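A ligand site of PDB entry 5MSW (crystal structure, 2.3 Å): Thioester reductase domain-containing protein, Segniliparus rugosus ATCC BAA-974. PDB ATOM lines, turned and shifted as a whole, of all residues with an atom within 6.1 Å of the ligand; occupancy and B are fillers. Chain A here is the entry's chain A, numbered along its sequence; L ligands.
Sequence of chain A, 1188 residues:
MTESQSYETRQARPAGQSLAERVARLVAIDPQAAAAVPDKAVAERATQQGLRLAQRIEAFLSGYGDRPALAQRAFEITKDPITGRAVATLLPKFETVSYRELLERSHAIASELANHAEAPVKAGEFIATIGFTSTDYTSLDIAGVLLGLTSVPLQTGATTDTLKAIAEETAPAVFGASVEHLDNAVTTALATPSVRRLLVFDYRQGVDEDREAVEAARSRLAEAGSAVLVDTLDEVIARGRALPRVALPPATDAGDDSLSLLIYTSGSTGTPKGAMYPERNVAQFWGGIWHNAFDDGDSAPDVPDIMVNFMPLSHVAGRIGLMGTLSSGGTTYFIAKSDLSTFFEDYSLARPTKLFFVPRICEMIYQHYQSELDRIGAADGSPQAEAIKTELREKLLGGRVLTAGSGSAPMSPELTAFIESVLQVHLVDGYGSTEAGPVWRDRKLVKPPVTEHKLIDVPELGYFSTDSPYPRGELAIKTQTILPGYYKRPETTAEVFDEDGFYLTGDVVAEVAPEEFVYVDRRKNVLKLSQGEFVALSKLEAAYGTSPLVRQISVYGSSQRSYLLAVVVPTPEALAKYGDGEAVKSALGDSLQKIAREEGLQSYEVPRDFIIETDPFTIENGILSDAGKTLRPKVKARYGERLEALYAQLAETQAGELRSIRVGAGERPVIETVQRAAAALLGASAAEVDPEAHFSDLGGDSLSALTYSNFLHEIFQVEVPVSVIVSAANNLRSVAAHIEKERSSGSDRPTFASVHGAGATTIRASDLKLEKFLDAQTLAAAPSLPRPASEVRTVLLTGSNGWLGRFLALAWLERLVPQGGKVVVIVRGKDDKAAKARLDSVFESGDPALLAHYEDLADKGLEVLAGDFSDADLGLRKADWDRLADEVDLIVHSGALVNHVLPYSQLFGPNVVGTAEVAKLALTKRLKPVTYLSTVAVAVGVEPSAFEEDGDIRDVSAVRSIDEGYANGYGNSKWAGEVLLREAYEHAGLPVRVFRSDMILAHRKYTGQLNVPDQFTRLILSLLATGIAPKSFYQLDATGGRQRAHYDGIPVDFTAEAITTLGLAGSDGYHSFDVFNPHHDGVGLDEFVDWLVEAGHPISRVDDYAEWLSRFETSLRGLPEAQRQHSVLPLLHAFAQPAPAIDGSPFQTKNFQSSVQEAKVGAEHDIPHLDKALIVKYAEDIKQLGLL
An oxygen (O5) of the ligand is in hydrogen-bond range of the side-chain amino group of Lys 629 (3.3 Å). O6 of the ligand sits at hydrogen-bond distance from NH1 of Arg 522, at 2.7 Å. A nitrogen (N3) of the ligand sits at hydrogen-bond distance from the backbone carbonyl oxygen of Gly 430 (2.7 Å). An oxygen (O3) of the ligand is in hydrogen-bond range of the backbone NH (N) of Thr 434, 3.4 Å away. The side-chain hydroxyl of Tyr 519 is in hydrogen-bond range of an oxygen (O7) of the ligand (2.8 Å). N3 of the ligand lies within hydrogen-bond range of OD1 of Asp 429 (3.2 Å). The side-chain hydroxyl of Thr 434 is in hydrogen-bond range of an oxygen (O3) of the ligand (3.2 Å). A nitrogen (N2) of the ligand sits at hydrogen-bond distance from the backbone NH of Ser 408 (3.3 Å). OD2 of Asp 507 lies within hydrogen-bond range of O6 of the ligand (2.5 Å).
The backbone carbonyl oxygen (O) of Ala 409 sits close to a nitrogen (N4) of the ligand (3.5 Å). OE1 of Glu 435 lies close to O3 of the ligand (3.4 Å). Merely in contact with the ligand: Thr 265, His 315, Gly 407, Pro 410, Tyr 431 and Gly 432. Within 4 Å of the ligand: Thr 265, His 315, Gly 407, Ser 408, Ala 409, Pro 410, Asp 429, Gly 430, Tyr 431, Gly 432, Thr 434, Glu 435, Asp 507, Tyr 519, Arg 522 and Lys 629. The nearest printed residue that does not touch the ligand is Ser 433 (4.03 Å).
N of Glu 435 lies close to OG of Ser 433 (3.3 Å). OD1 of Asp 507 is in salt-bridge range of NH1 of Arg 522. The backbone NH (N) of Gly 430 is in hydrogen-bond range of the backbone carbonyl oxygen (O) of Ser 406. N of Asp 507 sits close to OG1 of Thr 505, 3.2 Å away. The side-chain hydroxyl of Tyr 519 is in hydrogen-bond range of the backbone NH of Arg 522, 3.2 Å away. N of Tyr 431 lies within hydrogen-bond range of O of Trp 440.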
ATOM      1  N   THR A 265      15.619  32.188  27.535  1.00  0.00           N
ATOM      2  CA  THR A 265      17.076  32.087  27.359  1.00  0.00           C
ATOM      3  C   THR A 265      17.906  32.532  28.569  1.00  0.00           C
ATOM      4  O   THR A 265      18.661  31.740  29.128  1.00  0.00           O
ATOM      5  CB  THR A 265      17.560  32.955  26.162  1.00  0.00           C
ATOM      6  OG1 THR A 265      16.520  33.080  25.183  1.00  0.00           O
ATOM      7  CG2 THR A 265      18.808  32.380  25.506  1.00  0.00           C
ATOM      8  N   HIS A 315      14.705  23.635  25.733  1.00  0.00           N
ATOM      9  CA  HIS A 315      15.967  24.109  25.149  1.00  0.00           C
ATOM     10  C   HIS A 315      16.078  23.663  23.712  1.00  0.00           C
ATOM     11  O   HIS A 315      15.696  22.547  23.367  1.00  0.00           O
ATOM     12  CB  HIS A 315      17.123  23.536  25.972  1.00  0.00           C
ATOM     13  CG  HIS A 315      18.440  24.153  25.668  1.00  0.00           C
ATOM     14  ND1 HIS A 315      19.338  23.601  24.775  1.00  0.00           N
ATOM     15  CD2 HIS A 315      19.028  25.275  26.151  1.00  0.00           C
ATOM     16  CE1 HIS A 315      20.421  24.352  24.724  1.00  0.00           C
ATOM     17  NE2 HIS A 315      20.258  25.380  25.541  1.00  0.00           N
ATOM     18  N   VAL A 316      16.601  24.504  22.865  1.00  0.00           N
ATOM     19  CA  VAL A 316      16.639  24.186  21.454  1.00  0.00           C
ATOM     20  C   VAL A 316      17.340  22.869  21.104  1.00  0.00           C
ATOM     21  O   VAL A 316      17.044  22.292  20.057  1.00  0.00           O
ATOM     22  CB  VAL A 316      17.283  25.307  20.594  1.00  0.00           C
ATOM     23  CG1 VAL A 316      16.385  26.530  20.590  1.00  0.00           C
ATOM     24  CG2 VAL A 316      18.704  25.683  21.058  1.00  0.00           C
ATOM     25  N   SER A 406      28.664  17.349  19.392  1.00  0.00           N
ATOM     26  CA  SER A 406      28.483  18.083  20.617  1.00  0.00           C
ATOM     27  C   SER A 406      28.300  19.561  20.382  1.00  0.00           C
ATOM     28  O   SER A 406      28.768  20.092  19.386  1.00  0.00           O
ATOM     29  CB  SER A 406      29.672  17.903  21.562  1.00  0.00           C
ATOM     30  OG  SER A 406      29.449  18.622  22.791  1.00  0.00           O
ATOM     31  N   GLY A 407      27.640  20.212  21.334  1.00  0.00           N
ATOM     32  CA  GLY A 407      27.438  21.622  21.303  1.00  0.00           C
ATOM     33  C   GLY A 407      26.855  22.172  22.595  1.00  0.00           C
ATOM     34  O   GLY A 407      26.952  21.542  23.654  1.00  0.00           O
ATOM     35  N   SER A 408      26.343  23.385  22.498  1.00  0.00           N
ATOM     36  CA  SER A 408      25.789  24.149  23.601  1.00  0.00           C
ATOM     37  C   SER A 408      26.831  24.717  24.622  1.00  0.00           C
ATOM     38  O   SER A 408      26.504  25.668  25.324  1.00  0.00           O
ATOM     39  CB  SER A 408      24.644  23.362  24.313  1.00  0.00           C
ATOM     40  OG  SER A 408      25.102  22.617  25.443  1.00  0.00           O
ATOM     41  N   ALA A 409      28.040  24.175  24.718  1.00  0.00           N
ATOM     42  CA  ALA A 409      29.059  24.723  25.664  1.00  0.00           C
ATOM     43  C   ALA A 409      30.406  24.243  25.170  1.00  0.00           C
ATOM     44  O   ALA A 409      30.418  23.322  24.354  1.00  0.00           O
ATOM     45  CB  ALA A 409      28.813  24.265  27.094  1.00  0.00           C
ATOM     46  N   PRO A 410      31.510  24.836  25.677  1.00  0.00           N
ATOM     47  CA  PRO A 410      32.850  24.495  25.185  1.00  0.00           C
ATOM     48  C   PRO A 410      33.402  23.185  25.732  1.00  0.00           C
ATOM     49  O   PRO A 410      33.146  22.834  26.871  1.00  0.00           O
ATOM     50  CB  PRO A 410      33.714  25.656  25.664  1.00  0.00           C
ATOM     51  CG  PRO A 410      33.024  26.104  26.897  1.00  0.00           C
ATOM     52  CD  PRO A 410      31.570  26.008  26.564  1.00  0.00           C
ATOM     53  N   MET A 411      34.166  22.493  24.891  1.00  0.00           N
ATOM     54  CA  MET A 411      34.737  21.212  25.216  1.00  0.00           C
ATOM     55  C   MET A 411      36.246  21.399  25.306  1.00  0.00           C
ATOM     56  O   MET A 411      36.852  21.945  24.416  1.00  0.00           O
ATOM     57  CB  MET A 411      34.391  20.205  24.130  1.00  0.00           C
ATOM     58  CG  MET A 411      34.626  18.777  24.569  1.00  0.00           C
ATOM     59  SD  MET A 411      33.144  17.863  25.008  1.00  0.00           S
ATOM     60  CE  MET A 411      32.436  17.774  23.373  1.00  0.00           C
ATOM     61  N   ASP A 429      31.916  19.332  16.330  1.00  0.00           N
ATOM     62  CA  ASP A 429      31.548  20.459  17.176  1.00  0.00           C
ATOM     63  C   ASP A 429      30.618  21.462  16.440  1.00  0.00           C
ATOM     64  O   ASP A 429      30.953  22.009  15.393  1.00  0.00           O
ATOM     65  CB  ASP A 429      32.779  21.146  17.713  1.00  0.00           C
ATOM     66  CG  ASP A 429      32.425  22.301  18.659  1.00  0.00           C
ATOM     67  OD1 ASP A 429      31.775  22.051  19.701  1.00  0.00           O
ATOM     68  OD2 ASP A 429      32.766  23.468  18.336  1.00  0.00           O
ATOM     69  N   GLY A 430      29.457  21.720  17.015  1.00  0.00           N
ATOM     70  CA  GLY A 430      28.458  22.664  16.468  1.00  0.00           C
ATOM     71  C   GLY A 430      28.251  23.833  17.422  1.00  0.00           C
ATOM     72  O   GLY A 430      27.859  23.606  18.571  1.00  0.00           O
ATOM     73  N   TYR A 431      28.559  25.047  16.976  1.00  0.00           N
ATOM     74  CA  TYR A 431      28.386  26.270  17.713  1.00  0.00           C
ATOM     75  C   TYR A 431      27.136  26.919  17.163  1.00  0.00           C
ATOM     76  O   TYR A 431      26.940  27.021  15.964  1.00  0.00           O
ATOM     77  CB  TYR A 431      29.611  27.226  17.578  1.00  0.00           C
ATOM     78  CG  TYR A 431      29.271  28.613  18.037  1.00  0.00           C
ATOM     79  CD1 TYR A 431      29.129  28.895  19.393  1.00  0.00           C
ATOM     80  CD2 TYR A 431      28.978  29.617  17.109  1.00  0.00           C
ATOM     81  CE1 TYR A 431      28.723  30.141  19.814  1.00  0.00           C
ATOM     82  CE2 TYR A 431      28.567  30.868  17.518  1.00  0.00           C
ATOM     83  CZ  TYR A 431      28.437  31.132  18.876  1.00  0.00           C
ATOM     84  OH  TYR A 431      28.020  32.361  19.345  1.00  0.00           O
ATOM     85  N   GLY A 432      26.306  27.408  18.063  1.00  0.00           N
ATOM     86  CA  GLY A 432      25.016  27.956  17.694  1.00  0.00           C
ATOM     87  C   GLY A 432      24.329  28.503  18.929  1.00  0.00           C
ATOM     88  O   GLY A 432      24.895  28.468  20.020  1.00  0.00           O
ATOM     89  N   SER A 433      23.117  29.006  18.757  1.00  0.00           N
ATOM     90  CA  SER A 433      22.421  29.691  19.818  1.00  0.00           C
ATOM     91  C   SER A 433      20.948  29.696  19.534  1.00  0.00           C
ATOM     92  O   SER A 433      20.525  29.586  18.403  1.00  0.00           O
ATOM     93  CB  SER A 433      22.906  31.128  19.940  1.00  0.00           C
ATOM     94  OG  SER A 433      22.355  31.922  18.892  1.00  0.00           O
ATOM     95  N   THR A 434      20.155  29.867  20.579  1.00  0.00           N
ATOM     96  CA  THR A 434      18.745  30.084  20.469  1.00  0.00           C
ATOM     97  C   THR A 434      18.431  31.237  19.486  1.00  0.00           C
ATOM     98  O   THR A 434      17.610  31.092  18.593  1.00  0.00           O
ATOM     99  CB  THR A 434      18.162  30.354  21.847  1.00  0.00           C
ATOM    100  OG1 THR A 434      18.458  29.236  22.669  1.00  0.00           O
ATOM    101  CG2 THR A 434      16.664  30.524  21.787  1.00  0.00           C
ATOM    102  N   GLU A 435      19.166  32.325  19.642  1.00  0.00           N
ATOM    103  CA  GLU A 435      18.991  33.541  18.864  1.00  0.00           C
ATOM    104  C   GLU A 435      19.299  33.418  17.408  1.00  0.00           C
ATOM    105  O   GLU A 435      18.543  33.914  16.598  1.00  0.00           O
ATOM    106  CB  GLU A 435      19.857  34.678  19.424  1.00  0.00           C
ATOM    107  CG  GLU A 435      19.346  35.199  20.755  1.00  0.00           C
ATOM    108  CD  GLU A 435      19.810  34.434  21.973  1.00  0.00           C
ATOM    109  OE1 GLU A 435      20.359  33.311  21.859  1.00  0.00           O
ATOM    110  OE2 GLU A 435      19.606  34.995  23.059  1.00  0.00           O
ATOM    111  N   TRP A 440      28.354  27.717  13.373  1.00  0.00           N
ATOM    112  CA  TRP A 440      29.438  26.969  12.751  1.00  0.00           C
ATOM    113  C   TRP A 440      29.436  25.488  13.110  1.00  0.00           C
ATOM    114  O   TRP A 440      28.790  25.089  14.096  1.00  0.00           O
ATOM    115  CB  TRP A 440      30.801  27.591  13.028  1.00  0.00           C
ATOM    116  CG  TRP A 440      31.491  27.378  14.376  1.00  0.00           C
ATOM    117  CD1 TRP A 440      31.842  26.204  14.935  1.00  0.00           C
ATOM    118  CD2 TRP A 440      31.955  28.415  15.262  1.00  0.00           C
ATOM    119  NE1 TRP A 440      32.503  26.436  16.126  1.00  0.00           N
ATOM    120  CE2 TRP A 440      32.591  27.776  16.346  1.00  0.00           C
ATOM    121  CE3 TRP A 440      31.907  29.826  15.230  1.00  0.00           C
ATOM    122  CZ2 TRP A 440      33.204  28.500  17.405  1.00  0.00           C
ATOM    123  CZ3 TRP A 440      32.493  30.543  16.281  1.00  0.00           C
ATOM    124  CH2 TRP A 440      33.124  29.878  17.354  1.00  0.00           C
ATOM    125  N   THR A 505      26.713  38.365  19.000  1.00  0.00           N
ATOM    126  CA  THR A 505      26.566  37.098  19.678  1.00  0.00           C
ATOM    127  C   THR A 505      26.827  37.127  21.181  1.00  0.00           C
ATOM    128  O   THR A 505      26.386  36.199  21.874  1.00  0.00           O
ATOM    129  CB  THR A 505      27.457  36.033  19.059  1.00  0.00           C
ATOM    130  OG1 THR A 505      28.794  36.468  19.074  1.00  0.00           O
ATOM    131  CG2 THR A 505      27.028  35.729  17.636  1.00  0.00           C
ATOM    132  N   ASP A 507      29.782  36.647  22.105  1.00  0.00           N
ATOM    133  CA  ASP A 507      30.760  35.579  22.205  1.00  0.00           C
ATOM    134  C   ASP A 507      32.060  36.013  21.585  1.00  0.00           C
ATOM    135  O   ASP A 507      32.063  36.425  20.420  1.00  0.00           O
ATOM    136  CB  ASP A 507      30.245  34.334  21.504  1.00  0.00           C
ATOM    137  CG  ASP A 507      29.120  33.627  22.279  1.00  0.00           C
ATOM    138  OD1 ASP A 507      29.090  33.736  23.527  1.00  0.00           O
ATOM    139  OD2 ASP A 507      28.273  32.980  21.640  1.00  0.00           O
ATOM    140  N   TYR A 519      36.145  29.221  19.677  1.00  0.00           N
ATOM    141  CA  TYR A 519      35.499  29.928  20.777  1.00  0.00           C
ATOM    142  C   TYR A 519      36.494  30.169  21.950  1.00  0.00           C
ATOM    143  O   TYR A 519      37.241  29.287  22.327  1.00  0.00           O
ATOM    144  CB  TYR A 519      34.306  29.078  21.218  1.00  0.00           C
ATOM    145  CG  TYR A 519      33.441  29.584  22.354  1.00  0.00           C
ATOM    146  CD1 TYR A 519      32.255  30.281  22.085  1.00  0.00           C
ATOM    147  CD2 TYR A 519      33.738  29.279  23.664  1.00  0.00           C
ATOM    148  CE1 TYR A 519      31.421  30.703  23.099  1.00  0.00           C
ATOM    149  CE2 TYR A 519      32.901  29.657  24.675  1.00  0.00           C
ATOM    150  CZ  TYR A 519      31.754  30.398  24.393  1.00  0.00           C
ATOM    151  OH  TYR A 519      30.913  30.802  25.418  1.00  0.00           O
ATOM    152  N   ASP A 521      35.278  32.716  24.808  1.00  0.00           N
ATOM    153  CA  ASP A 521      34.243  32.716  25.863  1.00  0.00           C
ATOM    154  C   ASP A 521      33.154  33.708  25.598  1.00  0.00           C
ATOM    155  O   ASP A 521      33.296  34.614  24.758  1.00  0.00           O
ATOM    156  CB  ASP A 521      34.852  33.053  27.246  1.00  0.00           C
ATOM    157  CG  ASP A 521      34.349  32.139  28.354  1.00  0.00           C
ATOM    158  OD1 ASP A 521      33.219  31.615  28.221  1.00  0.00           O
ATOM    159  OD2 ASP A 521      35.074  31.940  29.370  1.00  0.00           O
ATOM    160  N   ARG A 522      32.080  33.583  26.358  1.00  0.00           N
ATOM    161  CA  ARG A 522      31.135  34.694  26.449  1.00  0.00           C
ATOM    162  C   ARG A 522      31.865  35.896  27.092  1.00  0.00           C
ATOM    163  O   ARG A 522      32.730  35.763  28.002  1.00  0.00           O
ATOM    164  CB  ARG A 522      29.883  34.360  27.264  1.00  0.00           C
ATOM    165  CG  ARG A 522      28.992  33.304  26.669  1.00  0.00           C
ATOM    166  CD  ARG A 522      27.600  33.349  27.254  1.00  0.00           C
ATOM    167  NE  ARG A 522      26.829  34.517  26.787  1.00  0.00           N
ATOM    168  CZ  ARG A 522      26.278  34.640  25.580  1.00  0.00           C
ATOM    169  NH1 ARG A 522      26.407  33.698  24.660  1.00  0.00           N
ATOM    170  NH2 ARG A 522      25.586  35.733  25.288  1.00  0.00           N
ATOM    171  N   LYS A 629      24.170  23.096  31.665  1.00  0.00           N
ATOM    172  CA  LYS A 629      25.274  24.068  31.888  1.00  0.00           C
ATOM    173  C   LYS A 629      25.259  24.536  33.318  1.00  0.00           C
ATOM    174  O   LYS A 629      24.234  24.636  33.909  1.00  0.00           O
ATOM    175  CB  LYS A 629      25.187  25.276  30.965  1.00  0.00           C
ATOM    176  CG  LYS A 629      25.603  24.974  29.536  1.00  0.00           C
ATOM    177  CD  LYS A 629      24.985  25.952  28.547  1.00  0.00           C
ATOM    178  CE  LYS A 629      25.686  27.308  28.568  1.00  0.00           C
ATOM    179  NZ  LYS A 629      25.202  28.170  27.446  1.00  0.00           N
HETATM  180  P1  LIG L   1      21.678  29.328  24.430  1.00  0.00           P
HETATM  181  O1  LIG L   1      21.721  28.066  23.581  1.00  0.00           O
HETATM  182  O2  LIG L   1      21.136  29.041  25.830  1.00  0.00           O
HETATM  183  O3  LIG L   1      21.077  30.577  23.825  1.00  0.00           O
HETATM  184  O4  LIG L   1      23.205  29.732  24.548  1.00  0.00           O
HETATM  185  C1  LIG L   1      24.116  29.524  23.475  1.00  0.00           C
HETATM  186  C2  LIG L   1      25.519  29.869  23.949  1.00  0.00           C
HETATM  187  O5  LIG L   1      26.186  28.666  24.361  1.00  0.00           O
HETATM  188  C3  LIG L   1      26.442  30.483  22.883  1.00  0.00           C
HETATM  189  O6  LIG L   1      26.248  31.874  22.678  1.00  0.00           O
HETATM  190  C4  LIG L   1      27.803  30.153  23.468  1.00  0.00           C
HETATM  191  O7  LIG L   1      28.220  31.041  24.524  1.00  0.00           O
HETATM  192  C5  LIG L   1      27.570  28.761  24.015  1.00  0.00           C
HETATM  193  N1  LIG L   1      27.853  27.723  23.004  1.00  0.00           N
HETATM  194  C6  LIG L   1      26.928  27.182  22.189  1.00  0.00           C
HETATM  195  N2  LIG L   1      27.481  26.265  21.403  1.00  0.00           N
HETATM  196  C7  LIG L   1      28.776  26.179  21.711  1.00  0.00           C
HETATM  197  C8  LIG L   1      29.924  25.361  21.255  1.00  0.00           C
HETATM  198  N3  LIG L   1      29.756  24.435  20.289  1.00  0.00           N
HETATM  199  N4  LIG L   1      31.133  25.603  21.817  1.00  0.00           N
HETATM  200  C9  LIG L   1      31.311  26.552  22.782  1.00  0.00           C
HETATM  201  N5  LIG L   1      30.288  27.292  23.272  1.00  0.00           N
HETATM  202  C10 LIG L   1      29.035  27.156  22.779  1.00  0.00           C
